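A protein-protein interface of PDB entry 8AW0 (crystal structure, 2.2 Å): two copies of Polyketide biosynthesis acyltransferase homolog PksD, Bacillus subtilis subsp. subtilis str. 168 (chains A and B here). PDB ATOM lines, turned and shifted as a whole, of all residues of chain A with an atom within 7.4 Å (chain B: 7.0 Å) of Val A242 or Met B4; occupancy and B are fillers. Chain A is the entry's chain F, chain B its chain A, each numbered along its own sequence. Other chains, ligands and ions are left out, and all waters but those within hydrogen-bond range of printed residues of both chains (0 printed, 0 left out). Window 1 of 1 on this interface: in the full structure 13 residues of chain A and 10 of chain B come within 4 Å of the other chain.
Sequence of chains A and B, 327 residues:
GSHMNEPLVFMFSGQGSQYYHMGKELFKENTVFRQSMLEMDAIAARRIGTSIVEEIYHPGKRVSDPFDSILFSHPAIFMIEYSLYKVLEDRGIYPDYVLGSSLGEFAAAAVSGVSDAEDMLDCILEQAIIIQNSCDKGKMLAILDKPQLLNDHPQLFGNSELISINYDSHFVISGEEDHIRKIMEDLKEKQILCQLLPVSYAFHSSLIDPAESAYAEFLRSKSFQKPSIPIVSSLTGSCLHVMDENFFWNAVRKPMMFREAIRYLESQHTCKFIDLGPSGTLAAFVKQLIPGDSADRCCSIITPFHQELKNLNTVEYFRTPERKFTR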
ATOM      1  N   LYS A 226      11.474  -3.454  10.786  1.00  0.00           N
ATOM      2  CA  LYS A 226      11.552  -3.934  12.157  1.00  0.00           C
ATOM      3  C   LYS A 226      11.048  -2.860  13.117  1.00  0.00           C
ATOM      4  O   LYS A 226      11.225  -1.658  12.862  1.00  0.00           O
ATOM      5  CB  LYS A 226      12.988  -4.333  12.518  1.00  0.00           C
ATOM      6  CG  LYS A 226      13.610  -5.442  11.671  1.00  0.00           C
ATOM      7  CD  LYS A 226      12.627  -6.589  11.436  1.00  0.00           C
ATOM      8  CE  LYS A 226      13.366  -7.917  11.222  1.00  0.00           C
ATOM      9  NZ  LYS A 226      14.360  -8.238  12.313  1.00  0.00           N
ATOM     10  N   PRO A 227      10.404  -3.245  14.219  1.00  0.00           N
ATOM     11  CA  PRO A 227      10.069  -2.272  15.265  1.00  0.00           C
ATOM     12  C   PRO A 227      11.322  -1.636  15.847  1.00  0.00           C
ATOM     13  O   PRO A 227      12.336  -2.306  16.051  1.00  0.00           O
ATOM     14  CB  PRO A 227       9.348  -3.119  16.318  1.00  0.00           C
ATOM     15  CG  PRO A 227       8.877  -4.327  15.588  1.00  0.00           C
ATOM     16  CD  PRO A 227       9.886  -4.592  14.522  1.00  0.00           C
ATOM     17  N   CYS A 239       5.517  -9.051  24.303  1.00  0.00           N
ATOM     18  CA  CYS A 239       6.327  -8.174  23.478  1.00  0.00           C
ATOM     19  C   CYS A 239       6.491  -8.783  22.091  1.00  0.00           C
ATOM     20  O   CYS A 239       6.459 -10.004  21.920  1.00  0.00           O
ATOM     21  CB  CYS A 239       7.687  -7.956  24.143  1.00  0.00           C
ATOM     22  SG  CYS A 239       8.633  -6.670  23.406  1.00  0.00           S
ATOM     23  N   LEU A 240       6.652  -7.927  21.087  1.00  0.00           N
ATOM     24  CA  LEU A 240       6.642  -8.362  19.696  1.00  0.00           C
ATOM     25  C   LEU A 240       7.829  -7.774  18.951  1.00  0.00           C
ATOM     26  O   LEU A 240       8.070  -6.563  19.023  1.00  0.00           O
ATOM     27  CB  LEU A 240       5.334  -7.959  19.009  1.00  0.00           C
ATOM     28  CG  LEU A 240       4.945  -8.794  17.788  1.00  0.00           C
ATOM     29  CD1 LEU A 240       4.526 -10.203  18.200  1.00  0.00           C
ATOM     30  CD2 LEU A 240       3.829  -8.099  17.036  1.00  0.00           C
ATOM     31  N   HIS A 241       8.557  -8.628  18.217  1.00  0.00           N
ATOM     32  CA  HIS A 241       9.756  -8.165  17.515  1.00  0.00           C
ATOM     33  C   HIS A 241       9.832  -8.619  16.069  1.00  0.00           C
ATOM     34  O   HIS A 241      10.345  -7.878  15.230  1.00  0.00           O
ATOM     35  CB  HIS A 241      11.013  -8.630  18.253  1.00  0.00           C
ATOM     36  CG  HIS A 241      11.163  -8.016  19.605  1.00  0.00           C
ATOM     37  ND1 HIS A 241      11.612  -6.725  19.790  1.00  0.00           N
ATOM     38  CD2 HIS A 241      10.893  -8.505  20.838  1.00  0.00           C
ATOM     39  CE1 HIS A 241      11.627  -6.451  21.082  1.00  0.00           C
ATOM     40  NE2 HIS A 241      11.195  -7.514  21.738  1.00  0.00           N
ATOM     41  N   VAL A 242       9.353  -9.817  15.755  1.00  0.00           N
ATOM     42  CA  VAL A 242       9.404 -10.344  14.398  1.00  0.00           C
ATOM     43  C   VAL A 242       7.985 -10.720  13.996  1.00  0.00           C
ATOM     44  O   VAL A 242       7.406 -11.668  14.543  1.00  0.00           O
ATOM     45  CB  VAL A 242      10.359 -11.538  14.277  1.00  0.00           C
ATOM     46  CG1 VAL A 242      10.472 -11.972  12.830  1.00  0.00           C
ATOM     47  CG2 VAL A 242      11.736 -11.167  14.814  1.00  0.00           C
ATOM     48  N   MET A 243       7.425  -9.982  13.043  1.00  0.00           N
ATOM     49  CA  MET A 243       6.045 -10.179  12.624  1.00  0.00           C
ATOM     50  C   MET A 243       5.971 -11.114  11.427  1.00  0.00           C
ATOM     51  O   MET A 243       6.773 -11.012  10.495  1.00  0.00           O
ATOM     52  CB  MET A 243       5.404  -8.843  12.257  1.00  0.00           C
ATOM     53  CG  MET A 243       5.672  -7.741  13.242  1.00  0.00           C
ATOM     54  SD  MET A 243       4.713  -6.271  12.843  1.00  0.00           S
ATOM     55  CE  MET A 243       5.153  -5.246  14.241  1.00  0.00           C
ATOM     56  N   ASP A 244       4.989 -12.012  11.447  1.00  0.00           N
ATOM     57  CA  ASP A 244       4.723 -12.815  10.268  1.00  0.00           C
ATOM     58  C   ASP A 244       4.044 -11.959   9.197  1.00  0.00           C
ATOM     59  O   ASP A 244       3.702 -10.791   9.413  1.00  0.00           O
ATOM     60  CB  ASP A 244       3.866 -14.034  10.622  1.00  0.00           C
ATOM     61  CG  ASP A 244       2.505 -13.655  11.198  1.00  0.00           C
ATOM     62  OD1 ASP A 244       2.456 -13.129  12.332  1.00  0.00           O
ATOM     63  OD2 ASP A 244       1.480 -13.895  10.518  1.00  0.00           O
ATOM     64  N   GLU A 245       3.858 -12.553   8.015  1.00  0.00           N
ATOM     65  CA  GLU A 245       3.223 -11.829   6.920  1.00  0.00           C
ATOM     66  C   GLU A 245       1.783 -11.447   7.249  1.00  0.00           C
ATOM     67  O   GLU A 245       1.298 -10.408   6.788  1.00  0.00           O
ATOM     68  CB  GLU A 245       3.256 -12.671   5.643  1.00  0.00           C
ATOM     69  CG  GLU A 245       4.618 -13.243   5.292  1.00  0.00           C
ATOM     70  CD  GLU A 245       4.528 -14.337   4.242  1.00  0.00           C
ATOM     71  OE1 GLU A 245       3.410 -14.593   3.742  1.00  0.00           O
ATOM     72  OE2 GLU A 245       5.575 -14.939   3.916  1.00  0.00           O
ATOM     73  N   PHE A 247       0.338 -10.528  10.067  1.00  0.00           N
ATOM     74  CA  PHE A 247       0.120  -9.833  11.333  1.00  0.00           C
ATOM     75  C   PHE A 247      -1.022  -8.828  11.231  1.00  0.00           C
ATOM     76  O   PHE A 247      -1.915  -8.794  12.084  1.00  0.00           O
ATOM     77  CB  PHE A 247       1.391  -9.130  11.783  1.00  0.00           C
ATOM     78  CG  PHE A 247       1.179  -8.206  12.940  1.00  0.00           C
ATOM     79  CD1 PHE A 247       0.988  -8.712  14.213  1.00  0.00           C
ATOM     80  CD2 PHE A 247       1.140  -6.835  12.753  1.00  0.00           C
ATOM     81  CE1 PHE A 247       0.785  -7.860  15.285  1.00  0.00           C
ATOM     82  CE2 PHE A 247       0.935  -5.977  13.822  1.00  0.00           C
ATOM     83  CZ  PHE A 247       0.759  -6.488  15.086  1.00  0.00           C
ATOM     84  N   MET B   4       7.029 -18.722   7.677  1.00  0.00           N
ATOM     85  CA  MET B   4       7.630 -17.491   8.188  1.00  0.00           C
ATOM     86  C   MET B   4       9.137 -17.667   8.166  1.00  0.00           C
ATOM     87  O   MET B   4       9.614 -18.787   8.297  1.00  0.00           O
ATOM     88  CB  MET B   4       7.138 -17.183   9.614  1.00  0.00           C
ATOM     89  CG  MET B   4       7.635 -15.876  10.257  1.00  0.00           C
ATOM     90  SD  MET B   4       6.944 -15.620  11.919  1.00  0.00           S
ATOM     91  CE  MET B   4       7.824 -14.170  12.473  1.00  0.00           C
ATOM     92  N   ASN B   5       9.895 -16.583   7.993  1.00  0.00           N
ATOM     93  CA  ASN B   5      11.338 -16.681   8.185  1.00  0.00           C
ATOM     94  C   ASN B   5      11.614 -16.979   9.650  1.00  0.00           C
ATOM     95  O   ASN B   5      11.169 -16.240  10.533  1.00  0.00           O
ATOM     96  CB  ASN B   5      12.039 -15.391   7.755  1.00  0.00           C
ATOM     97  CG  ASN B   5      11.758 -15.018   6.310  1.00  0.00           C
ATOM     98  OD1 ASN B   5      12.473 -15.444   5.401  1.00  0.00           O
ATOM     99  ND2 ASN B   5      10.721 -14.219   6.091  1.00  0.00           N
ATOM    100  N   GLU B   6      12.307 -18.081   9.911  1.00  0.00           N
ATOM    101  CA  GLU B   6      12.657 -18.447  11.282  1.00  0.00           C
ATOM    102  C   GLU B   6      13.755 -17.524  11.809  1.00  0.00           C
ATOM    103  O   GLU B   6      14.824 -17.433  11.190  1.00  0.00           O
ATOM    104  CB  GLU B   6      13.109 -19.902  11.331  1.00  0.00           C
ATOM    105  CG  GLU B   6      12.242 -20.831  10.495  1.00  0.00           C
ATOM    106  CD  GLU B   6      12.876 -22.195  10.282  1.00  0.00           C
ATOM    107  OE1 GLU B   6      13.308 -22.822  11.279  1.00  0.00           O
ATOM    108  OE2 GLU B   6      12.968 -22.624   9.107  1.00  0.00           O
ATOM    109  N   PRO B   7      13.540 -16.831  12.926  1.00  0.00           N
ATOM    110  CA  PRO B   7      14.528 -15.852  13.404  1.00  0.00           C
ATOM    111  C   PRO B   7      15.800 -16.501  13.937  1.00  0.00           C
ATOM    112  O   PRO B   7      15.775 -17.589  14.522  1.00  0.00           O
ATOM    113  CB  PRO B   7      13.784 -15.117  14.529  1.00  0.00           C
ATOM    114  CG  PRO B   7      12.327 -15.471  14.340  1.00  0.00           C
ATOM    115  CD  PRO B   7      12.326 -16.842  13.753  1.00  0.00           C
ATOM    116  N   ASP B  96      18.526 -11.954  14.775  1.00  0.00           N
ATOM    117  CA  ASP B  96      17.238 -11.352  15.092  1.00  0.00           C
ATOM    118  C   ASP B  96      17.098 -11.112  16.589  1.00  0.00           C
ATOM    119  O   ASP B  96      16.495 -10.115  17.004  1.00  0.00           O
ATOM    120  CB  ASP B  96      16.118 -12.238  14.573  1.00  0.00           C
ATOM    121  CG  ASP B  96      16.061 -12.246  13.070  1.00  0.00           C
ATOM    122  OD1 ASP B  96      15.874 -11.153  12.493  1.00  0.00           O
ATOM    123  OD2 ASP B  96      16.226 -13.330  12.466  1.00  0.00           O
ATOM    124  N   TYR B  97      17.660 -12.007  17.408  1.00  0.00           N
ATOM    125  CA  TYR B  97      17.776 -11.821  18.849  1.00  0.00           C
ATOM    126  C   TYR B  97      19.190 -12.172  19.292  1.00  0.00           C
ATOM    127  O   TYR B  97      19.894 -12.943  18.633  1.00  0.00           O
ATOM    128  CB  TYR B  97      16.809 -12.712  19.642  1.00  0.00           C
ATOM    129  CG  TYR B  97      15.325 -12.533  19.407  1.00  0.00           C
ATOM    130  CD1 TYR B  97      14.700 -13.122  18.316  1.00  0.00           C
ATOM    131  CD2 TYR B  97      14.532 -11.837  20.320  1.00  0.00           C
ATOM    132  CE1 TYR B  97      13.332 -12.998  18.119  1.00  0.00           C
ATOM    133  CE2 TYR B  97      13.166 -11.702  20.134  1.00  0.00           C
ATOM    134  CZ  TYR B  97      12.571 -12.286  19.029  1.00  0.00           C
ATOM    135  OH  TYR B  97      11.209 -12.166  18.829  1.00  0.00           O
ATOM    136  N   PRO B 230      16.953  -6.991  19.781  1.00  0.00           N
ATOM    137  CA  PRO B 230      16.281  -7.539  20.968  1.00  0.00           C
ATOM    138  C   PRO B 230      17.220  -8.450  21.744  1.00  0.00           C
ATOM    139  O   PRO B 230      17.834  -9.359  21.181  1.00  0.00           O
ATOM    140  CB  PRO B 230      15.097  -8.313  20.379  1.00  0.00           C
ATOM    141  CG  PRO B 230      14.862  -7.683  19.020  1.00  0.00           C
ATOM    142  CD  PRO B 230      16.215  -7.281  18.534  1.00  0.00           C
ATOM    143  N   GLN B 268       6.719 -17.642  20.691  1.00  0.00           N
ATOM    144  CA  GLN B 268       6.237 -16.766  19.629  1.00  0.00           C
ATOM    145  C   GLN B 268       6.634 -17.221  18.235  1.00  0.00           C
ATOM    146  O   GLN B 268       5.949 -16.871  17.269  1.00  0.00           O
ATOM    147  CB  GLN B 268       6.734 -15.335  19.854  1.00  0.00           C
ATOM    148  CG  GLN B 268       6.215 -14.698  21.137  1.00  0.00           C
ATOM    149  CD  GLN B 268       4.692 -14.818  21.341  1.00  0.00           C
ATOM    150  OE1 GLN B 268       3.926 -15.104  20.413  1.00  0.00           O
ATOM    151  NE2 GLN B 268       4.261 -14.622  22.583  1.00  0.00           N
ATOM    152  N   HIS B 269       7.702 -17.994  18.109  1.00  0.00           N
ATOM    153  CA  HIS B 269       8.140 -18.495  16.815  1.00  0.00           C
ATOM    154  C   HIS B 269       9.141 -19.631  16.966  1.00  0.00           C
ATOM    155  O   HIS B 269       9.701 -19.840  18.045  1.00  0.00           O
ATOM    156  CB  HIS B 269       8.672 -17.330  15.961  1.00  0.00           C
ATOM    157  CG  HIS B 269       9.365 -16.267  16.752  1.00  0.00           C
ATOM    158  ND1 HIS B 269      10.640 -16.403  17.244  1.00  0.00           N
ATOM    159  CD2 HIS B 269       8.967 -15.014  17.079  1.00  0.00           C
ATOM    160  CE1 HIS B 269      10.979 -15.302  17.891  1.00  0.00           C
ATOM    161  NE2 HIS B 269       9.985 -14.438  17.795  1.00  0.00           N
ATOM    162  N   THR B 270       9.311 -20.407  15.904  1.00  0.00           N
ATOM    163  CA  THR B 270      10.238 -21.533  15.872  1.00  0.00           C
ATOM    164  C   THR B 270      11.613 -20.991  15.477  1.00  0.00           C
ATOM    165  O   THR B 270      11.882 -20.755  14.296  1.00  0.00           O
ATOM    166  CB  THR B 270       9.727 -22.589  14.898  1.00  0.00           C
ATOM    167  OG1 THR B 270       8.391 -22.962  15.256  1.00  0.00           O
ATOM    168  CG2 THR B 270      10.580 -23.827  14.940  1.00  0.00           C
ATOM    169  N   PRO B 321      15.869 -16.254   3.691  1.00  0.00           N
ATOM    170  CA  PRO B 321      15.674 -16.053   2.244  1.00  0.00           C
ATOM    171  C   PRO B 321      15.408 -14.591   1.896  1.00  0.00           C
ATOM    172  O   PRO B 321      15.279 -13.715   2.754  1.00  0.00           O
ATOM    173  CB  PRO B 321      14.438 -16.927   1.938  1.00  0.00           C
ATOM    174  CG  PRO B 321      14.430 -17.978   3.019  1.00  0.00           C
ATOM    175  CD  PRO B 321      14.984 -17.316   4.240  1.00  0.00           C
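No position is printed for both chains. Of the 6 pairs that touch across the chains among the printed residues, none has its exchanged pair printed and touching as well.
The side-chain hydroxyl (OH) of Tyr B97 lies within hydrogen-bond range of a ring nitrogen (NE2) of His B269 (2.8 Å).
Pro A227 touches none of the printed residues of chain B. Val A242 touches just one residue of chain B: Met B4. Printed residues of chain B within 4 Å of Asp A244: Met B4 (3.7 Å). Of chain A, only Val A242 (3.3 Å), Met A243 (3.7 Å) and Asp A244 (3.7 Å) come within 4 Å of Met B4. Printed residues of chain A within 4 Å of Tyr B97: His A241 (3.6 Å). Of the printed residues of chain A, Pro B230 touches His A241 (3.5 Å). The nearest residue of chain A that does not touch Met B4 is Glu A245 (5.4 Å).
Hydrophobic or aromatic side chains of chain A within 4 Å of the printed part of chain B: His A241 and Val A242. Along chain A the printed residues that touch a printed residue of chain B span positions 226 to 244. Printed residues of chain B that touch a printed residue of chain A: Met B4, Asp B96, Tyr B97 and Pro B230. Hydrophobic or aromatic side chains of chain B that line the printed part of chain A: Met B4, Tyr B97 and Pro B230. Among the printed residues, Asp or Glu carboxylates within 4 Å of a Lys or Arg side-chain nitrogen of the other chain: Lys A226 with Asp B96 (3.3 Å).
Among the printed residues, merely in contact across the chains: His A241 with Tyr B97 (3.6 Å), His A241 with Pro B230 (3.5 Å), Val A242 with Met B4 (3.3 Å), Met A243 with Met B4 (3.7 Å) and Asp A244 with Met B4 (3.7 Å).
The side-chain amino group (NZ) of Lys A226 is in salt-bridge range of the side-chain carboxylate (OD1) of Asp B96 (3.3 Å).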
